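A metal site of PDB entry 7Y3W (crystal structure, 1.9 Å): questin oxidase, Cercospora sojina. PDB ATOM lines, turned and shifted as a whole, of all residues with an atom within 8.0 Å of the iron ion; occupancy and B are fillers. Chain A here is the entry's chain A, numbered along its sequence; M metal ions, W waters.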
ATOM      1  N   ALA A  51     -21.105   1.928  19.967  1.00  0.00           N
ATOM      2  CA  ALA A  51     -20.235   1.691  18.776  1.00  0.00           C
ATOM      3  C   ALA A  51     -20.217   2.937  17.849  1.00  0.00           C
ATOM      4  O   ALA A  51     -20.122   2.840  16.609  1.00  0.00           O
ATOM      5  CB  ALA A  51     -20.717   0.453  18.090  1.00  0.00           C
ATOM      6  N   HIS A  53     -17.935   5.546  17.831  1.00  0.00           N
ATOM      7  CA  HIS A  53     -16.628   6.267  17.903  1.00  0.00           C
ATOM      8  C   HIS A  53     -16.320   6.880  16.530  1.00  0.00           C
ATOM      9  O   HIS A  53     -16.589   6.213  15.494  1.00  0.00           O
ATOM     10  CB  HIS A  53     -15.505   5.346  18.390  1.00  0.00           C
ATOM     11  CG  HIS A  53     -15.903   4.498  19.551  1.00  0.00           C
ATOM     12  ND1 HIS A  53     -16.572   3.303  19.378  1.00  0.00           N
ATOM     13  CD2 HIS A  53     -15.689   4.641  20.864  1.00  0.00           C
ATOM     14  CE1 HIS A  53     -16.800   2.788  20.566  1.00  0.00           C
ATOM     15  NE2 HIS A  53     -16.283   3.586  21.493  1.00  0.00           N
ATOM     16  N   ASN A  54     -15.880   8.129  16.527  1.00  0.00           N
ATOM     17  CA  ASN A  54     -15.427   8.805  15.283  1.00  0.00           C
ATOM     18  C   ASN A  54     -14.040   8.286  14.896  1.00  0.00           C
ATOM     19  O   ASN A  54     -13.070   8.552  15.636  1.00  0.00           O
ATOM     20  CB  ASN A  54     -15.499  10.346  15.433  1.00  0.00           C
ATOM     21  CG  ASN A  54     -14.933  11.090  14.231  1.00  0.00           C
ATOM     22  OD1 ASN A  54     -14.623  10.501  13.211  1.00  0.00           O
ATOM     23  ND2 ASN A  54     -14.827  12.413  14.364  1.00  0.00           N
ATOM     24  N   HIS A  55     -13.924   7.536  13.788  1.00  0.00           N
ATOM     25  CA  HIS A  55     -12.645   6.884  13.366  1.00  0.00           C
ATOM     26  C   HIS A  55     -11.840   7.774  12.398  1.00  0.00           C
ATOM     27  O   HIS A  55     -10.777   7.352  11.905  1.00  0.00           O
ATOM     28  CB  HIS A  55     -12.940   5.542  12.697  1.00  0.00           C
ATOM     29  CG  HIS A  55     -13.268   4.473  13.682  1.00  0.00           C
ATOM     30  ND1 HIS A  55     -14.410   4.533  14.449  1.00  0.00           N
ATOM     31  CD2 HIS A  55     -12.667   3.308  13.948  1.00  0.00           C
ATOM     32  CE1 HIS A  55     -14.454   3.457  15.205  1.00  0.00           C
ATOM     33  NE2 HIS A  55     -13.408   2.689  14.921  1.00  0.00           N
ATOM     34  N   HIS A  58      -8.133   8.157  12.966  1.00  0.00           N
ATOM     35  CA  HIS A  58      -7.491   6.821  12.839  1.00  0.00           C
ATOM     36  C   HIS A  58      -7.260   6.504  11.356  1.00  0.00           C
ATOM     37  O   HIS A  58      -6.142   6.035  10.977  1.00  0.00           O
ATOM     38  CB  HIS A  58      -8.386   5.715  13.395  1.00  0.00           C
ATOM     39  CG  HIS A  58      -8.939   5.922  14.755  1.00  0.00           C
ATOM     40  ND1 HIS A  58      -9.840   5.025  15.279  1.00  0.00           N
ATOM     41  CD2 HIS A  58      -8.803   6.918  15.646  1.00  0.00           C
ATOM     42  CE1 HIS A  58     -10.184   5.424  16.485  1.00  0.00           C
ATOM     43  NE2 HIS A  58      -9.539   6.565  16.760  1.00  0.00           N
ATOM     44  N   HIS A  83     -19.389   9.024  10.360  1.00  0.00           N
ATOM     45  CA  HIS A  83     -18.810   9.162  11.706  1.00  0.00           C
ATOM     46  C   HIS A  83     -18.737  10.636  12.110  1.00  0.00           C
ATOM     47  O   HIS A  83     -18.303  10.903  13.245  1.00  0.00           O
ATOM     48  CB  HIS A  83     -17.405   8.583  11.787  1.00  0.00           C
ATOM     49  CG  HIS A  83     -17.292   7.109  11.596  1.00  0.00           C
ATOM     50  ND1 HIS A  83     -16.205   6.405  12.065  1.00  0.00           N
ATOM     51  CD2 HIS A  83     -18.129   6.200  11.049  1.00  0.00           C
ATOM     52  CE1 HIS A  83     -16.337   5.131  11.746  1.00  0.00           C
ATOM     53  NE2 HIS A  83     -17.511   4.971  11.120  1.00  0.00           N
ATOM     54  N   GLY A 155     -14.936   0.407  25.205  1.00  0.00           N
ATOM     55  CA  GLY A 155     -15.488   0.312  23.848  1.00  0.00           C
ATOM     56  C   GLY A 155     -14.579  -0.406  22.865  1.00  0.00           C
ATOM     57  O   GLY A 155     -14.514   0.027  21.700  1.00  0.00           O
ATOM     58  N   ALA A 156     -13.916  -1.475  23.311  1.00  0.00           N
ATOM     59  CA  ALA A 156     -12.922  -2.209  22.510  1.00  0.00           C
ATOM     60  C   ALA A 156     -11.798  -1.255  22.097  1.00  0.00           C
ATOM     61  O   ALA A 156     -11.348  -1.350  20.953  1.00  0.00           O
ATOM     62  CB  ALA A 156     -13.565  -2.893  21.309  1.00  0.00           C
ATOM     63  N   TYR A 157     -11.298  -0.433  23.046  1.00  0.00           N
ATOM     64  CA  TYR A 157      -9.939   0.179  23.069  1.00  0.00           C
ATOM     65  C   TYR A 157      -9.891   1.468  22.251  1.00  0.00           C
ATOM     66  O   TYR A 157      -8.768   1.992  22.032  1.00  0.00           O
ATOM     67  CB  TYR A 157      -8.874  -0.789  22.564  1.00  0.00           C
ATOM     68  CG  TYR A 157      -8.867  -2.106  23.295  1.00  0.00           C
ATOM     69  CD1 TYR A 157      -8.573  -2.173  24.651  1.00  0.00           C
ATOM     70  CD2 TYR A 157      -9.135  -3.284  22.630  1.00  0.00           C
ATOM     71  CE1 TYR A 157      -8.542  -3.387  25.313  1.00  0.00           C
ATOM     72  CE2 TYR A 157      -9.088  -4.509  23.280  1.00  0.00           C
ATOM     73  CZ  TYR A 157      -8.807  -4.556  24.619  1.00  0.00           C
ATOM     74  OH  TYR A 157      -8.806  -5.774  25.253  1.00  0.00           O
ATOM     75  N   HIS A 158     -11.048   2.029  21.904  1.00  0.00           N
ATOM     76  CA  HIS A 158     -11.115   3.313  21.168  1.00  0.00           C
ATOM     77  C   HIS A 158     -10.438   4.469  21.912  1.00  0.00           C
ATOM     78  O   HIS A 158      -9.703   5.186  21.236  1.00  0.00           O
ATOM     79  CB  HIS A 158     -12.523   3.606  20.673  1.00  0.00           C
ATOM     80  CG  HIS A 158     -12.913   2.668  19.568  1.00  0.00           C
ATOM     81  ND1 HIS A 158     -13.592   1.491  19.798  1.00  0.00           N
ATOM     82  CD2 HIS A 158     -12.647   2.694  18.246  1.00  0.00           C
ATOM     83  CE1 HIS A 158     -13.803   0.878  18.648  1.00  0.00           C
ATOM     84  NE2 HIS A 158     -13.177   1.563  17.659  1.00  0.00           N
ATOM     85  N   ILE A 161      -6.726   3.916  21.497  1.00  0.00           N
ATOM     86  CA  ILE A 161      -6.297   4.179  20.088  1.00  0.00           C
ATOM     87  C   ILE A 161      -6.216   5.678  19.838  1.00  0.00           C
ATOM     88  O   ILE A 161      -5.188   6.126  19.273  1.00  0.00           O
ATOM     89  CB  ILE A 161      -7.256   3.451  19.127  1.00  0.00           C
ATOM     90  CG1 ILE A 161      -7.015   1.945  19.164  1.00  0.00           C
ATOM     91  CG2 ILE A 161      -7.171   4.010  17.723  1.00  0.00           C
ATOM     92  CD1 ILE A 161      -8.229   1.116  18.766  1.00  0.00           C
ATOM     93  N   PHE A 292     -14.851  -8.761  14.301  1.00  0.00           N
ATOM     94  CA  PHE A 292     -14.772  -7.273  14.484  1.00  0.00           C
ATOM     95  C   PHE A 292     -14.081  -6.910  15.788  1.00  0.00           C
ATOM     96  O   PHE A 292     -13.273  -5.983  15.817  1.00  0.00           O
ATOM     97  CB  PHE A 292     -16.186  -6.698  14.454  1.00  0.00           C
ATOM     98  CG  PHE A 292     -16.285  -5.201  14.524  1.00  0.00           C
ATOM     99  CD1 PHE A 292     -15.963  -4.421  13.417  1.00  0.00           C
ATOM    100  CD2 PHE A 292     -16.727  -4.579  15.678  1.00  0.00           C
ATOM    101  CE1 PHE A 292     -16.096  -3.035  13.446  1.00  0.00           C
ATOM    102  CE2 PHE A 292     -16.851  -3.199  15.705  1.00  0.00           C
ATOM    103  CZ  PHE A 292     -16.569  -2.440  14.592  1.00  0.00           C
ATOM    104  N   MET A 295     -10.383  -8.032  15.945  1.00  0.00           N
ATOM    105  CA  MET A 295      -9.638  -7.110  15.105  1.00  0.00           C
ATOM    106  C   MET A 295      -9.212  -5.890  15.927  1.00  0.00           C
ATOM    107  O   MET A 295      -8.073  -5.410  15.784  1.00  0.00           O
ATOM    108  CB  MET A 295     -10.463  -6.738  13.873  1.00  0.00           C
ATOM    109  CG  MET A 295      -9.844  -5.608  13.033  1.00  0.00           C
ATOM    110  SD  MET A 295     -10.587  -3.854  13.568  1.00  0.00           S
ATOM    111  CE  MET A 295     -12.440  -4.087  12.885  1.00  0.00           C
ATOM    112  N   HIS A 296     -10.098  -5.385  16.788  1.00  0.00           N
ATOM    113  CA  HIS A 296      -9.767  -4.303  17.704  1.00  0.00           C
ATOM    114  C   HIS A 296      -8.657  -4.694  18.686  1.00  0.00           C
ATOM    115  O   HIS A 296      -7.880  -3.856  19.146  1.00  0.00           O
ATOM    116  CB  HIS A 296     -10.995  -3.738  18.430  1.00  0.00           C
ATOM    117  CG  HIS A 296     -11.814  -2.853  17.560  1.00  0.00           C
ATOM    118  ND1 HIS A 296     -12.670  -3.360  16.607  1.00  0.00           N
ATOM    119  CD2 HIS A 296     -11.836  -1.510  17.435  1.00  0.00           C
ATOM    120  CE1 HIS A 296     -13.212  -2.342  15.957  1.00  0.00           C
ATOM    121  NE2 HIS A 296     -12.694  -1.207  16.425  1.00  0.00           N
ATOM    122  N   THR A 299      -5.710  -4.086  16.431  1.00  0.00           N
ATOM    123  CA  THR A 299      -5.495  -2.682  16.024  1.00  0.00           C
ATOM    124  C   THR A 299      -4.924  -1.866  17.187  1.00  0.00           C
ATOM    125  O   THR A 299      -4.012  -1.091  16.928  1.00  0.00           O
ATOM    126  CB  THR A 299      -6.735  -1.961  15.500  1.00  0.00           C
ATOM    127  OG1 THR A 299      -7.767  -1.922  16.488  1.00  0.00           O
ATOM    128  CG2 THR A 299      -7.195  -2.589  14.193  1.00  0.00           C
ATOM    129  N   ASP A 372     -13.580   2.235   6.584  1.00  0.00           N
ATOM    130  CA  ASP A 372     -13.734   3.239   7.654  1.00  0.00           C
ATOM    131  C   ASP A 372     -12.438   3.442   8.431  1.00  0.00           C
ATOM    132  O   ASP A 372     -12.466   4.224   9.380  1.00  0.00           O
ATOM    133  CB  ASP A 372     -14.868   2.850   8.604  1.00  0.00           C
ATOM    134  CG  ASP A 372     -14.757   1.459   9.211  1.00  0.00           C
ATOM    135  OD1 ASP A 372     -13.752   0.769   8.945  1.00  0.00           O
ATOM    136  OD2 ASP A 372     -15.703   1.082   9.942  1.00  0.00           O
ATOM    137  N   GLY A 373     -11.349   2.751   8.065  1.00  0.00           N
ATOM    138  CA  GLY A 373     -10.072   2.868   8.770  1.00  0.00           C
ATOM    139  C   GLY A 373      -9.615   1.534   9.396  1.00  0.00           C
ATOM    140  O   GLY A 373      -8.380   1.350   9.559  1.00  0.00           O
ATOM    141  N   HIS A 374     -10.519   0.594   9.648  1.00  0.00           N
ATOM    142  CA  HIS A 374     -10.137  -0.651  10.365  1.00  0.00           C
ATOM    143  C   HIS A 374      -9.123  -1.460   9.549  1.00  0.00           C
ATOM    144  O   HIS A 374      -8.212  -2.040  10.171  1.00  0.00           O
ATOM    145  CB  HIS A 374     -11.355  -1.457  10.773  1.00  0.00           C
ATOM    146  CG  HIS A 374     -12.128  -0.805  11.840  1.00  0.00           C
ATOM    147  ND1 HIS A 374     -13.355  -0.242  11.611  1.00  0.00           N
ATOM    148  CD2 HIS A 374     -11.842  -0.591  13.148  1.00  0.00           C
ATOM    149  CE1 HIS A 374     -13.812   0.269  12.752  1.00  0.00           C
ATOM    150  NE2 HIS A 374     -12.948   0.021  13.713  1.00  0.00           N
ATOM    151  N   KCX A 377      -5.707   0.107   9.882  1.00  0.00           N
ATOM    152  CA  KCX A 377      -5.258  -0.090  11.238  1.00  0.00           C
ATOM    153  CB  KCX A 377      -6.352   0.246  12.243  1.00  0.00           C
ATOM    154  CG  KCX A 377      -6.602   1.726  12.367  1.00  0.00           C
ATOM    155  CD  KCX A 377      -7.950   1.995  12.982  1.00  0.00           C
ATOM    156  CE  KCX A 377      -7.854   1.932  14.479  1.00  0.00           C
ATOM    157  NZ  KCX A 377      -9.159   2.001  15.061  1.00  0.00           N
ATOM    158  C   KCX A 377      -4.788  -1.516  11.497  1.00  0.00           C
ATOM    159  O   KCX A 377      -3.759  -1.716  12.152  1.00  0.00           O
ATOM    160  CX  KCX A 377      -9.834   0.910  15.436  1.00  0.00           C
ATOM    161  OQ1 KCX A 377     -11.022   1.200  15.945  1.00  0.00           O
ATOM    162  OQ2 KCX A 377      -9.409  -0.229  15.328  1.00  0.00           O
HETATM  163 FE    FE M   1     -13.001   0.764  15.749  1.00  0.00          FE
HETATM  164  O   HOH W   1     -15.115   0.421  15.630  1.00  0.00           O
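The backbone carbonyl oxygen (O) of Phe 292 is in hydrogen-bond range of a ring nitrogen (ND1) of His 296 (2.8 Å). The backbone carbonyl oxygen (O) of Gly 155 is in hydrogen-bond range of a ring nitrogen (ND1) of His 158, at 2.6 Å. ND1 of His 374 sits at hydrogen-bond distance from OD1 of Asp 372, 2.9 Å away. The backbone carbonyl oxygen (O) of His 53 lies within hydrogen-bond range of a ring nitrogen (ND1) of His 55. The backbone NH (N) of His 55 sits at hydrogen-bond distance from a ring nitrogen (ND1) of His 83 (3.1 Å). ND1 of His 296 is in hydrogen-bond range of SD of Met 295. OQ2 of KCX 377 sits close to OG1 of Thr 299, at 2.6 Å. NZ of KCX 377 sits close to ND1 of His 58, 3.1 Å away.
Of the 19 residues printed, 5 come within 4 Å of the iron ion. The nearest printed residue that does not touch the iron ion is Phe 292 (4.9 Å).
The iron ion is bound by OQ1 of KCX 377 (2.0 Å), NE2 of His 158 (2.1 Å), NE2 of His 296 (2.1 Å), NE2 of His 55 (2.1 Å), water W1 (2.1 Å) and NE2 of His 374 (2.2 Å).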
